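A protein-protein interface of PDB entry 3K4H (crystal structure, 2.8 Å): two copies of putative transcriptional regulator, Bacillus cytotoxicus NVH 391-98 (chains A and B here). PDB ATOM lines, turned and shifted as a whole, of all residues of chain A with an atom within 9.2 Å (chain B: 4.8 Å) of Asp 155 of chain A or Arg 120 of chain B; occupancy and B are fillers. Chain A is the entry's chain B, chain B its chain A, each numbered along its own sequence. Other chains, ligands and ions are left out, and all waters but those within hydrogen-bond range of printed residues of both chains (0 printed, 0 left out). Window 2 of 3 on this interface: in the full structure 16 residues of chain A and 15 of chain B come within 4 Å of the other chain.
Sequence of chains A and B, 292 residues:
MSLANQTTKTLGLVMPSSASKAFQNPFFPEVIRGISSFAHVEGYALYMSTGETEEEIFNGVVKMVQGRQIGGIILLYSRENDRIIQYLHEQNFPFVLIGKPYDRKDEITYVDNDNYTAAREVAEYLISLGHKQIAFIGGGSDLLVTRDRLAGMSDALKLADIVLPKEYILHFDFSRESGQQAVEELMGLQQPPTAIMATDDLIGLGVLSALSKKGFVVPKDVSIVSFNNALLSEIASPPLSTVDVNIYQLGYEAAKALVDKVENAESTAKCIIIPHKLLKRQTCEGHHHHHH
OH of Tyr 116 of chain B lies within hydrogen-bond range of NH2 of Arg 120 of chain A (2.5 Å).
The guanidinium group of Arg 120 of chain B is in hydrogen-bond range of the side-chain hydroxyl of Tyr 116 of chain A (2.6 Å).
NH2 of Arg 120 of chain B lies within salt-bridge range of OD2 of Asp 155 of chain A, at 2.6 Å.
The side-chain carboxylate (OD2) of Asp 155 of chain B is in salt-bridge range of the guanidinium group (NH2) of Arg 120 of chain A (2.4 Å).
OH of Tyr 116 of chain B is in hydrogen-bond range of NE of Arg 120 of chain B, 3.4 Å away.
The side-chain hydroxyl (OH) of Tyr 116 of chain B lies within hydrogen-bond range of the side-chain carboxylate (OD2) of Asp 155 of chain B, at 2.5 Å.
The guanidinium group (NH1) of Arg 120 of chain B is in salt-bridge range of the side-chain carboxylate (OE2) of Glu 124 of chain B (3.4 Å).
OH of Tyr 116 of chain A lies within hydrogen-bond range of NE of Arg 120 of chain A (3.4 Å).
The side-chain carboxylate (OD2) of Asp 155 of chain A is in hydrogen-bond range of the side-chain hydroxyl (OH) of Tyr 116 of chain A (2.7 Å).
The side-chain carboxylate (OE2) of Glu 124 of chain A is in salt-bridge range of the guanidinium group (NH1) of Arg 120 of chain A (3.7 Å).
Leu 159 of chain B touches Asp 155 of chain A (CD2 to OD1, 3.6 Å).
Leu 159 of chain B touches Lys 158 of chain A (CD2 to CD, 3.5 Å).
OD1 of Asp 155 of chain B touches CD1 of Leu 159 of chain A, at 3.6 Å.
CD2 of Leu 159 of chain A touches CD2 of Leu 159 of chain B, 3.2 Å away.
Asp 155 of chain A touches just these residues of chain B: Arg 120 and Leu 159.
Arg 120 of chain B touches two residues of chain A.
No residue of chain A comes within 4 Å of Ala 119 of chain B.
No residue of chain A comes within 4 Å of Ala 123 of chain B.
Of the printed residues of chain B, Arg 120 of chain A touches Tyr 116 (2.5 Å) and Asp 155 (2.4 Å).
Of the printed residues of chain B, Lys 158 of chain A touches Leu 159 (3.5 Å).
Of the printed residues of chain B, Leu 159 of chain A touches Asp 155 (3.6 Å) and Leu 159 (3.2 Å).
Printed residues of chain A within 4 Å of Tyr 116 of chain B: Arg 120.
The nearest printed residue of chain B that does not touch Asp 155 of chain A is Tyr 116 of chain B (6.1 Å).
The nearest residue of chain A that does not touch Arg 120 of chain B is Arg 120 of chain A (4.8 Å).
The nearest printed residue of chain B that does not touch Arg 120 of chain A is Arg 120 of chain B (4.8 Å).
Among the printed residues, Asp or Glu carboxylates within 4 Å of a Lys or Arg side-chain nitrogen of the other chain: Arg 120 of chain A with Asp 155 of chain B and Asp 155 of chain A with Arg 120 of chain B.
Tyr 116 of chain A touches Arg 120 of chain B, and with the chains exchanged Arg 120 of chain A touches Tyr 116 of chain B.
Arg 120 of chain A touches Asp 155 of chain B, and with the chains exchanged Asp 155 of chain A touches Arg 120 of chain B.
Asp 155 of chain A touches Leu 159 of chain B, and with the chains exchanged Leu 159 of chain A touches Asp 155 of chain B.
Leu 159 of chain A touches its own counterpart, Leu 159 of chain B.
Of the 8 pairs that touch across the chains among the printed residues, 7 have their exchanged pair printed and touching as well.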
ATOM      1  N   TYR A 116      -7.467   8.125  34.896  1.00  0.00           N
ATOM      2  CA  TYR A 116      -7.305   9.181  33.955  1.00  0.00           C
ATOM      3  C   TYR A 116      -6.220  10.110  34.391  1.00  0.00           C
ATOM      4  O   TYR A 116      -5.400  10.485  33.630  1.00  0.00           O
ATOM      5  CB  TYR A 116      -8.593   9.954  33.821  1.00  0.00           C
ATOM      6  CG  TYR A 116      -8.465  11.198  33.015  1.00  0.00           C
ATOM      7  CD1 TYR A 116      -8.768  11.215  31.702  1.00  0.00           C
ATOM      8  CD2 TYR A 116      -8.047  12.353  33.574  1.00  0.00           C
ATOM      9  CE1 TYR A 116      -8.639  12.317  30.989  1.00  0.00           C
ATOM     10  CE2 TYR A 116      -7.916  13.447  32.857  1.00  0.00           C
ATOM     11  CZ  TYR A 116      -8.210  13.421  31.571  1.00  0.00           C
ATOM     12  OH  TYR A 116      -8.097  14.531  30.832  1.00  0.00           O
ATOM     13  N   THR A 117      -6.145  10.445  35.638  1.00  0.00           N
ATOM     14  CA  THR A 117      -5.082  11.309  36.046  1.00  0.00           C
ATOM     15  C   THR A 117      -3.740  10.687  35.849  1.00  0.00           C
ATOM     16  O   THR A 117      -2.799  11.319  35.484  1.00  0.00           O
ATOM     17  CB  THR A 117      -5.245  11.779  37.445  1.00  0.00           C
ATOM     18  OG1 THR A 117      -6.593  12.169  37.655  1.00  0.00           O
ATOM     19  CG2 THR A 117      -4.406  12.936  37.679  1.00  0.00           C
ATOM     20  N   ALA A 119      -2.606   8.636  33.741  1.00  0.00           N
ATOM     21  CA  ALA A 119      -2.184   8.707  32.373  1.00  0.00           C
ATOM     22  C   ALA A 119      -1.784  10.106  32.027  1.00  0.00           C
ATOM     23  O   ALA A 119      -0.881  10.319  31.287  1.00  0.00           O
ATOM     24  CB  ALA A 119      -3.224   8.193  31.477  1.00  0.00           C
ATOM     25  N   ARG A 120      -2.507  11.087  32.504  1.00  0.00           N
ATOM     26  CA  ARG A 120      -2.090  12.415  32.210  1.00  0.00           C
ATOM     27  C   ARG A 120      -0.732  12.658  32.820  1.00  0.00           C
ATOM     28  O   ARG A 120       0.140  13.184  32.207  1.00  0.00           O
ATOM     29  CB  ARG A 120      -3.070  13.371  32.859  1.00  0.00           C
ATOM     30  CG  ARG A 120      -4.173  13.849  31.985  1.00  0.00           C
ATOM     31  CD  ARG A 120      -3.983  15.287  31.630  1.00  0.00           C
ATOM     32  NE  ARG A 120      -5.210  16.024  31.815  1.00  0.00           N
ATOM     33  CZ  ARG A 120      -5.266  17.276  32.216  1.00  0.00           C
ATOM     34  NH1 ARG A 120      -4.161  17.933  32.464  1.00  0.00           N
ATOM     35  NH2 ARG A 120      -6.429  17.860  32.383  1.00  0.00           N
ATOM     36  N   GLU A 121      -0.528  12.197  34.025  1.00  0.00           N
ATOM     37  CA  GLU A 121       0.711  12.441  34.708  1.00  0.00           C
ATOM     38  C   GLU A 121       1.849  11.810  33.983  1.00  0.00           C
ATOM     39  O   GLU A 121       2.934  12.315  33.936  1.00  0.00           O
ATOM     40  CB  GLU A 121       0.627  12.000  36.142  1.00  0.00           C
ATOM     41  CG  GLU A 121       0.095  13.054  37.030  1.00  0.00           C
ATOM     42  CD  GLU A 121      -0.337  12.521  38.335  1.00  0.00           C
ATOM     43  OE1 GLU A 121      -0.763  11.393  38.363  1.00  0.00           O
ATOM     44  OE2 GLU A 121      -0.267  13.210  39.340  1.00  0.00           O
ATOM     45  N   ALA A 123       2.088  11.283  30.869  1.00  0.00           N
ATOM     46  CA  ALA A 123       2.340  11.989  29.611  1.00  0.00           C
ATOM     47  C   ALA A 123       3.171  13.234  29.855  1.00  0.00           C
ATOM     48  O   ALA A 123       4.172  13.457  29.180  1.00  0.00           O
ATOM     49  CB  ALA A 123       1.054  12.333  28.917  1.00  0.00           C
ATOM     50  N   GLU A 124       2.768  14.021  30.848  1.00  0.00           N
ATOM     51  CA  GLU A 124       3.465  15.262  31.206  1.00  0.00           C
ATOM     52  C   GLU A 124       4.917  14.980  31.575  1.00  0.00           C
ATOM     53  O   GLU A 124       5.800  15.794  31.325  1.00  0.00           O
ATOM     54  CB  GLU A 124       2.744  15.971  32.358  1.00  0.00           C
ATOM     55  CG  GLU A 124       1.256  16.275  32.089  1.00  0.00           C
ATOM     56  CD  GLU A 124       0.510  16.778  33.325  1.00  0.00           C
ATOM     57  OE1 GLU A 124       1.063  16.659  34.441  1.00  0.00           O
ATOM     58  OE2 GLU A 124      -0.631  17.281  33.174  1.00  0.00           O
ATOM     59  N   ILE A 127       6.732  14.356  28.241  1.00  0.00           N
ATOM     60  CA  ILE A 127       6.879  15.588  27.534  1.00  0.00           C
ATOM     61  C   ILE A 127       8.011  16.291  28.198  1.00  0.00           C
ATOM     62  O   ILE A 127       8.850  16.870  27.571  1.00  0.00           O
ATOM     63  CB  ILE A 127       5.658  16.429  27.693  1.00  0.00           C
ATOM     64  CG1 ILE A 127       4.433  15.631  27.329  1.00  0.00           C
ATOM     65  CG2 ILE A 127       5.705  17.542  26.757  1.00  0.00           C
ATOM     66  CD1 ILE A 127       4.240  15.513  25.902  1.00  0.00           C
ATOM     67  N   ARG A 147      -9.858   2.537  28.483  1.00  0.00           N
ATOM     68  CA  ARG A 147     -10.434   3.758  27.933  1.00  0.00           C
ATOM     69  C   ARG A 147      -9.944   4.988  28.679  1.00  0.00           C
ATOM     70  O   ARG A 147      -9.618   5.998  28.043  1.00  0.00           O
ATOM     71  CB  ARG A 147     -11.954   3.727  27.952  1.00  0.00           C
ATOM     72  CG  ARG A 147     -12.588   2.985  26.813  1.00  0.00           C
ATOM     73  CD  ARG A 147     -14.057   3.363  26.735  1.00  0.00           C
ATOM     74  NE  ARG A 147     -14.904   2.195  26.488  1.00  0.00           N
ATOM     75  CZ  ARG A 147     -16.099   2.000  27.047  1.00  0.00           C
ATOM     76  NH1 ARG A 147     -16.601   2.896  27.897  1.00  0.00           N
ATOM     77  NH2 ARG A 147     -16.794   0.901  26.760  1.00  0.00           N
ATOM     78  N   ASP A 148      -9.894   4.897  30.015  1.00  0.00           N
ATOM     79  CA  ASP A 148      -9.460   6.011  30.867  1.00  0.00           C
ATOM     80  C   ASP A 148      -7.983   6.322  30.685  1.00  0.00           C
ATOM     81  O   ASP A 148      -7.600   7.479  30.510  1.00  0.00           O
ATOM     82  CB  ASP A 148      -9.769   5.756  32.351  1.00  0.00           C
ATOM     83  CG  ASP A 148     -11.267   5.720  32.651  1.00  0.00           C
ATOM     84  OD1 ASP A 148     -11.650   5.360  33.784  1.00  0.00           O
ATOM     85  OD2 ASP A 148     -12.066   6.039  31.750  1.00  0.00           O
ATOM     86  N   ARG A 149      -7.150   5.293  30.711  1.00  0.00           N
ATOM     87  CA  ARG A 149      -5.720   5.490  30.502  1.00  0.00           C
ATOM     88  C   ARG A 149      -5.432   6.025  29.091  1.00  0.00           C
ATOM     89  O   ARG A 149      -4.500   6.805  28.905  1.00  0.00           O
ATOM     90  CB  ARG A 149      -4.946   4.216  30.841  1.00  0.00           C
ATOM     91  CG  ARG A 149      -4.962   3.918  32.338  1.00  0.00           C
ATOM     92  CD  ARG A 149      -4.492   2.493  32.690  1.00  0.00           C
ATOM     93  NE  ARG A 149      -4.520   2.261  34.141  1.00  0.00           N
ATOM     94  CZ  ARG A 149      -4.218   1.110  34.741  1.00  0.00           C
ATOM     95  NH1 ARG A 149      -3.861   0.047  34.033  1.00  0.00           N
ATOM     96  NH2 ARG A 149      -4.279   1.009  36.060  1.00  0.00           N
ATOM     97  N   LEU A 150      -6.260   5.650  28.112  1.00  0.00           N
ATOM     98  CA  LEU A 150      -6.171   6.244  26.770  1.00  0.00           C
ATOM     99  C   LEU A 150      -6.471   7.726  26.849  1.00  0.00           C
ATOM    100  O   LEU A 150      -5.649   8.555  26.453  1.00  0.00           O
ATOM    101  CB  LEU A 150      -7.154   5.587  25.781  1.00  0.00           C
ATOM    102  CG  LEU A 150      -6.805   5.358  24.288  1.00  0.00           C
ATOM    103  CD1 LEU A 150      -8.093   5.232  23.481  1.00  0.00           C
ATOM    104  CD2 LEU A 150      -5.871   6.406  23.662  1.00  0.00           C
ATOM    105  N   ALA A 151      -7.648   8.043  27.385  1.00  0.00           N
ATOM    106  CA  ALA A 151      -8.148   9.411  27.468  1.00  0.00           C
ATOM    107  C   ALA A 151      -7.178  10.337  28.185  1.00  0.00           C
ATOM    108  O   ALA A 151      -6.903  11.425  27.700  1.00  0.00           O
ATOM    109  CB  ALA A 151      -9.518   9.434  28.134  1.00  0.00           C
ATOM    110  N   GLY A 152      -6.648   9.888  29.324  1.00  0.00           N
ATOM    111  CA  GLY A 152      -5.675  10.650  30.098  1.00  0.00           C
ATOM    112  C   GLY A 152      -4.532  11.129  29.244  1.00  0.00           C
ATOM    113  O   GLY A 152      -4.207  12.302  29.243  1.00  0.00           O
ATOM    114  N   MET A 153      -3.939  10.212  28.490  1.00  0.00           N
ATOM    115  CA  MET A 153      -2.779  10.518  27.674  1.00  0.00           C
ATOM    116  C   MET A 153      -3.149  11.375  26.459  1.00  0.00           C
ATOM    117  O   MET A 153      -2.541  12.413  26.214  1.00  0.00           O
ATOM    118  CB  MET A 153      -2.126   9.222  27.223  1.00  0.00           C
ATOM    119  CG  MET A 153      -0.727   9.421  26.708  1.00  0.00           C
ATOM    120  SD  MET A 153      -0.064   8.000  25.525  1.00  0.00           S
ATOM    121  CE  MET A 153       1.729   7.936  26.278  1.00  0.00           C
ATOM    122  N   SER A 154      -4.151  10.929  25.709  1.00  0.00           N
ATOM    123  CA  SER A 154      -4.662  11.656  24.557  1.00  0.00           C
ATOM    124  C   SER A 154      -4.998  13.127  24.870  1.00  0.00           C
ATOM    125  O   SER A 154      -4.923  13.989  23.989  1.00  0.00           O
ATOM    126  CB  SER A 154      -5.887  10.926  23.995  1.00  0.00           C
ATOM    127  OG  SER A 154      -6.521  11.688  22.981  1.00  0.00           O
ATOM    128  N   ASP A 155      -5.366  13.399  26.123  1.00  0.00           N
ATOM    129  CA  ASP A 155      -5.640  14.751  26.592  1.00  0.00           C
ATOM    130  C   ASP A 155      -4.377  15.535  26.902  1.00  0.00           C
ATOM    131  O   ASP A 155      -4.260  16.688  26.506  1.00  0.00           O
ATOM    132  CB  ASP A 155      -6.568  14.743  27.806  1.00  0.00           C
ATOM    133  CG  ASP A 155      -8.028  14.601  27.422  1.00  0.00           C
ATOM    134  OD1 ASP A 155      -8.338  14.784  26.230  1.00  0.00           O
ATOM    135  OD2 ASP A 155      -8.872  14.303  28.301  1.00  0.00           O
ATOM    136  N   ALA A 156      -3.460  14.917  27.583  1.00  0.00           N
ATOM    137  CA  ALA A 156      -2.273  15.617  27.913  1.00  0.00           C
ATOM    138  C   ALA A 156      -1.597  15.958  26.637  1.00  0.00           C
ATOM    139  O   ALA A 156      -1.017  16.997  26.510  1.00  0.00           O
ATOM    140  CB  ALA A 156      -1.417  14.777  28.729  1.00  0.00           C
ATOM    141  N   LEU A 157      -1.599  15.059  25.683  1.00  0.00           N
ATOM    142  CA  LEU A 157      -0.967  15.416  24.448  1.00  0.00           C
ATOM    143  C   LEU A 157      -1.646  16.563  23.772  1.00  0.00           C
ATOM    144  O   LEU A 157      -1.024  17.489  23.353  1.00  0.00           O
ATOM    145  CB  LEU A 157      -1.074  14.241  23.507  1.00  0.00           C
ATOM    146  CG  LEU A 157       0.231  13.566  23.142  1.00  0.00           C
ATOM    147  CD1 LEU A 157       1.142  13.554  24.315  1.00  0.00           C
ATOM    148  CD2 LEU A 157      -0.052  12.191  22.671  1.00  0.00           C
ATOM    149  N   LYS A 158      -2.954  16.547  23.765  1.00  0.00           N
ATOM    150  CA  LYS A 158      -3.690  17.551  23.068  1.00  0.00           C
ATOM    151  C   LYS A 158      -3.422  18.878  23.668  1.00  0.00           C
ATOM    152  O   LYS A 158      -3.294  19.840  22.992  1.00  0.00           O
ATOM    153  CB  LYS A 158      -5.150  17.245  23.199  1.00  0.00           C
ATOM    154  CG  LYS A 158      -5.930  17.420  21.968  1.00  0.00           C
ATOM    155  CD  LYS A 158      -7.327  16.860  22.118  1.00  0.00           C
ATOM    156  CE  LYS A 158      -7.363  15.359  21.887  1.00  0.00           C
ATOM    157  NZ  LYS A 158      -8.693  14.822  21.492  1.00  0.00           N
ATOM    158  N   LEU A 159      -3.368  18.925  24.972  1.00  0.00           N
ATOM    159  CA  LEU A 159      -3.089  20.135  25.695  1.00  0.00           C
ATOM    160  C   LEU A 159      -1.723  20.574  25.339  1.00  0.00           C
ATOM    161  O   LEU A 159      -1.425  21.722  25.272  1.00  0.00           O
ATOM    162  CB  LEU A 159      -3.270  19.955  27.176  1.00  0.00           C
ATOM    163  CG  LEU A 159      -4.631  19.435  27.617  1.00  0.00           C
ATOM    164  CD1 LEU A 159      -4.868  19.799  29.010  1.00  0.00           C
ATOM    165  CD2 LEU A 159      -5.732  19.947  26.798  1.00  0.00           C
ATOM    166  N   ALA A 160      -0.866  19.601  25.220  1.00  0.00           N
ATOM    167  CA  ALA A 160       0.513  19.734  24.825  1.00  0.00           C
ATOM    168  C   ALA A 160       0.578  20.272  23.427  1.00  0.00           C
ATOM    169  O   ALA A 160       1.457  21.021  23.082  1.00  0.00           O
ATOM    170  CB  ALA A 160       1.183  18.444  24.909  1.00  0.00           C
ATOM    171  N   ASP A 161      -0.345  19.818  22.606  1.00  0.00           N
ATOM    172  CA  ASP A 161      -0.339  20.055  21.184  1.00  0.00           C
ATOM    173  C   ASP A 161       0.421  19.081  20.368  1.00  0.00           C
ATOM    174  O   ASP A 161       0.502  19.214  19.177  1.00  0.00           O
ATOM    175  CB  ASP A 161       0.292  21.393  20.931  1.00  0.00           C
ATOM    176  CG  ASP A 161      -0.358  22.116  19.806  1.00  0.00           C
ATOM    177  OD1 ASP A 161      -1.395  22.743  20.054  1.00  0.00           O
ATOM    178  OD2 ASP A 161       0.154  22.047  18.678  1.00  0.00           O
ATOM    179  N   ILE A 162       0.929  18.065  21.015  1.00  0.00           N
ATOM    180  CA  ILE A 162       1.464  16.915  20.344  1.00  0.00           C
ATOM    181  C   ILE A 162       0.316  16.181  19.746  1.00  0.00           C
ATOM    182  O   ILE A 162      -0.793  16.323  20.179  1.00  0.00           O
ATOM    183  CB  ILE A 162       2.193  16.006  21.235  1.00  0.00           C
ATOM    184  CG1 ILE A 162       3.336  16.756  21.862  1.00  0.00           C
ATOM    185  CG2 ILE A 162       2.697  14.871  20.437  1.00  0.00           C
ATOM    186  CD1 ILE A 162       3.066  18.166  21.908  1.00  0.00           C
ATOM    187  N   LEU A 164      -1.665  12.780  17.935  1.00  0.00           N
ATOM    188  CA  LEU A 164      -1.769  11.346  18.005  1.00  0.00           C
ATOM    189  C   LEU A 164      -2.355  10.766  16.762  1.00  0.00           C
ATOM    190  O   LEU A 164      -3.478  11.036  16.410  1.00  0.00           O
ATOM    191  CB  LEU A 164      -2.619  10.950  19.183  1.00  0.00           C
ATOM    192  CG  LEU A 164      -2.037   9.773  19.938  1.00  0.00           C
ATOM    193  CD1 LEU A 164      -1.034  10.229  20.942  1.00  0.00           C
ATOM    194  CD2 LEU A 164      -3.115   8.958  20.569  1.00  0.00           C
ATOM    195  N   TYR B 116     -13.159  18.232  39.406  1.00  0.00           N
ATOM    196  CA  TYR B 116     -12.521  18.429  38.121  1.00  0.00           C
ATOM    197  C   TYR B 116     -13.455  17.976  37.022  1.00  0.00           C
ATOM    198  O   TYR B 116     -13.739  18.738  36.095  1.00  0.00           O
ATOM    199  CB  TYR B 116     -11.196  17.689  38.025  1.00  0.00           C
ATOM    200  CG  TYR B 116     -10.546  17.853  36.684  1.00  0.00           C
ATOM    201  CD1 TYR B 116      -9.712  18.930  36.419  1.00  0.00           C
ATOM    202  CD2 TYR B 116     -10.794  16.942  35.659  1.00  0.00           C
ATOM    203  CE1 TYR B 116      -9.126  19.069  35.163  1.00  0.00           C
ATOM    204  CE2 TYR B 116     -10.230  17.078  34.429  1.00  0.00           C
ATOM    205  CZ  TYR B 116      -9.401  18.136  34.188  1.00  0.00           C
ATOM    206  OH  TYR B 116      -8.855  18.246  32.946  1.00  0.00           O
ATOM    207  N   THR B 117     -13.953  16.753  37.136  1.00  0.00           N
ATOM    208  CA  THR B 117     -14.852  16.224  36.134  1.00  0.00           C
ATOM    209  C   THR B 117     -16.233  16.883  36.123  1.00  0.00           C
ATOM    210  O   THR B 117     -16.837  17.035  35.052  1.00  0.00           O
ATOM    211  CB  THR B 117     -14.974  14.712  36.261  1.00  0.00           C
ATOM    212  OG1 THR B 117     -13.649  14.161  36.307  1.00  0.00           O
ATOM    213  CG2 THR B 117     -15.718  14.134  35.065  1.00  0.00           C
ATOM    214  N   ALA B 118     -16.744  17.278  37.292  1.00  0.00           N
ATOM    215  CA  ALA B 118     -18.053  17.921  37.291  1.00  0.00           C
ATOM    216  C   ALA B 118     -17.956  19.171  36.415  1.00  0.00           C
ATOM    217  O   ALA B 118     -18.773  19.334  35.510  1.00  0.00           O
ATOM    218  CB  ALA B 118     -18.532  18.229  38.678  1.00  0.00           C
ATOM    219  N   ALA B 119     -16.918  19.992  36.630  1.00  0.00           N
ATOM    220  CA  ALA B 119     -16.706  21.255  35.898  1.00  0.00           C
ATOM    221  C   ALA B 119     -16.408  21.020  34.425  1.00  0.00           C
ATOM    222  O   ALA B 119     -16.892  21.749  33.569  1.00  0.00           O
ATOM    223  CB  ALA B 119     -15.603  22.090  36.542  1.00  0.00           C
ATOM    224  N   ARG B 120     -15.620  20.003  34.126  1.00  0.00           N
ATOM    225  CA  ARG B 120     -15.433  19.589  32.753  1.00  0.00           C
ATOM    226  C   ARG B 120     -16.779  19.329  32.114  1.00  0.00           C
ATOM    227  O   ARG B 120     -17.017  19.757  31.001  1.00  0.00           O
ATOM    228  CB  ARG B 120     -14.590  18.302  32.688  1.00  0.00           C
ATOM    229  CG  ARG B 120     -13.122  18.514  32.484  1.00  0.00           C
ATOM    230  CD  ARG B 120     -12.749  18.244  31.047  1.00  0.00           C
ATOM    231  NE  ARG B 120     -11.512  17.461  30.939  1.00  0.00           N
ATOM    232  CZ  ARG B 120     -11.258  16.581  29.973  1.00  0.00           C
ATOM    233  NH1 ARG B 120     -12.137  16.349  29.008  1.00  0.00           N
ATOM    234  NH2 ARG B 120     -10.116  15.928  29.973  1.00  0.00           N
ATOM    235  N   GLU B 121     -17.657  18.615  32.817  1.00  0.00           N
ATOM    236  CA  GLU B 121     -18.921  18.187  32.238  1.00  0.00           C
ATOM    237  C   GLU B 121     -19.847  19.380  32.007  1.00  0.00           C
ATOM    238  O   GLU B 121     -20.476  19.491  30.940  1.00  0.00           O
ATOM    239  CB  GLU B 121     -19.595  17.155  33.118  1.00  0.00           C
ATOM    240  CG  GLU B 121     -19.049  15.745  32.999  1.00  0.00           C
ATOM    241  CD  GLU B 121     -19.546  14.843  34.122  1.00  0.00           C
ATOM    242  OE1 GLU B 121     -20.089  15.354  35.126  1.00  0.00           O
ATOM    243  OE2 GLU B 121     -19.387  13.614  34.017  1.00  0.00           O
ATOM    244  N   VAL B 122     -19.914  20.274  32.993  1.00  0.00           N
ATOM    245  CA  VAL B 122     -20.648  21.518  32.842  1.00  0.00           C
ATOM    246  C   VAL B 122     -20.145  22.304  31.617  1.00  0.00           C
ATOM    247  O   VAL B 122     -20.944  22.861  30.857  1.00  0.00           O
ATOM    248  CB  VAL B 122     -20.569  22.378  34.130  1.00  0.00           C
ATOM    249  CG1 VAL B 122     -21.100  23.771  33.900  1.00  0.00           C
ATOM    250  CG2 VAL B 122     -21.371  21.733  35.240  1.00  0.00           C
ATOM    251  N   ALA B 123     -18.825  22.348  31.424  1.00  0.00           N
ATOM    252  CA  ALA B 123     -18.264  23.140  30.348  1.00  0.00           C
ATOM    253  C   ALA B 123     -18.542  22.452  29.021  1.00  0.00           C
ATOM    254  O   ALA B 123     -18.833  23.121  28.020  1.00  0.00           O
ATOM    255  CB  ALA B 123     -16.781  23.377  30.555  1.00  0.00           C
ATOM    256  N   GLU B 124     -18.482  21.117  29.019  1.00  0.00           N
ATOM    257  CA  GLU B 124     -18.852  20.342  27.823  1.00  0.00           C
ATOM    258  C   GLU B 124     -20.314  20.607  27.461  1.00  0.00           C
ATOM    259  O   GLU B 124     -20.639  20.837  26.287  1.00  0.00           O
ATOM    260  CB  GLU B 124     -18.567  18.858  28.007  1.00  0.00           C
ATOM    261  CG  GLU B 124     -17.107  18.538  27.776  1.00  0.00           C
ATOM    262  CD  GLU B 124     -16.636  17.209  28.379  1.00  0.00           C
ATOM    263  OE1 GLU B 124     -17.476  16.318  28.696  1.00  0.00           O
ATOM    264  OE2 GLU B 124     -15.393  17.064  28.525  1.00  0.00           O
ATOM    265  N   GLY B 152     -11.003  22.106  35.562  1.00  0.00           N
ATOM    266  CA  GLY B 152     -11.872  21.324  34.684  1.00  0.00           C
ATOM    267  C   GLY B 152     -12.544  22.115  33.581  1.00  0.00           C
ATOM    268  O   GLY B 152     -12.642  21.641  32.464  1.00  0.00           O
ATOM    269  N   MET B 153     -13.021  23.318  33.877  1.00  0.00           N
ATOM    270  CA  MET B 153     -13.676  24.104  32.842  1.00  0.00           C
ATOM    271  C   MET B 153     -12.622  24.641  31.845  1.00  0.00           C
ATOM    272  O   MET B 153     -12.838  24.670  30.614  1.00  0.00           O
ATOM    273  CB  MET B 153     -14.499  25.239  33.452  1.00  0.00           C
ATOM    274  CG  MET B 153     -13.946  26.623  33.178  1.00  0.00           C
ATOM    275  SD  MET B 153     -15.359  27.957  33.010  1.00  0.00           S
ATOM    276  CE  MET B 153     -14.329  29.327  32.081  1.00  0.00           C
ATOM    277  N   ASP B 155      -9.601  23.283  31.094  1.00  0.00           N
ATOM    278  CA  ASP B 155      -9.149  22.214  30.202  1.00  0.00           C
ATOM    279  C   ASP B 155     -10.180  21.933  29.131  1.00  0.00           C
ATOM    280  O   ASP B 155      -9.838  21.757  27.964  1.00  0.00           O
ATOM    281  CB  ASP B 155      -8.844  20.915  30.969  1.00  0.00           C
ATOM    282  CG  ASP B 155      -7.506  20.956  31.705  1.00  0.00           C
ATOM    283  OD1 ASP B 155      -6.645  21.809  31.393  1.00  0.00           O
ATOM    284  OD2 ASP B 155      -7.317  20.129  32.616  1.00  0.00           O
ATOM    285  N   ALA B 156     -11.446  21.897  29.538  1.00  0.00           N
ATOM    286  CA  ALA B 156     -12.543  21.643  28.608  1.00  0.00           C
ATOM    287  C   ALA B 156     -12.527  22.665  27.469  1.00  0.00           C
ATOM    288  O   ALA B 156     -12.720  22.304  26.291  1.00  0.00           O
ATOM    289  CB  ALA B 156     -13.887  21.622  29.331  1.00  0.00           C
ATOM    290  N   LEU B 159      -9.551  22.074  25.152  1.00  0.00           N
ATOM    291  CA  LEU B 159      -9.709  20.870  24.362  1.00  0.00           C
ATOM    292  C   LEU B 159     -10.633  21.064  23.171  1.00  0.00           C
ATOM    293  O   LEU B 159     -10.538  20.339  22.198  1.00  0.00           O
ATOM    294  CB  LEU B 159     -10.132  19.673  25.238  1.00  0.00           C
ATOM    295  CG  LEU B 159      -8.988  19.104  26.108  1.00  0.00           C
ATOM    296  CD1 LEU B 159      -9.496  18.335  27.309  1.00  0.00           C
ATOM    297  CD2 LEU B 159      -7.994  18.260  25.297  1.00  0.00           C
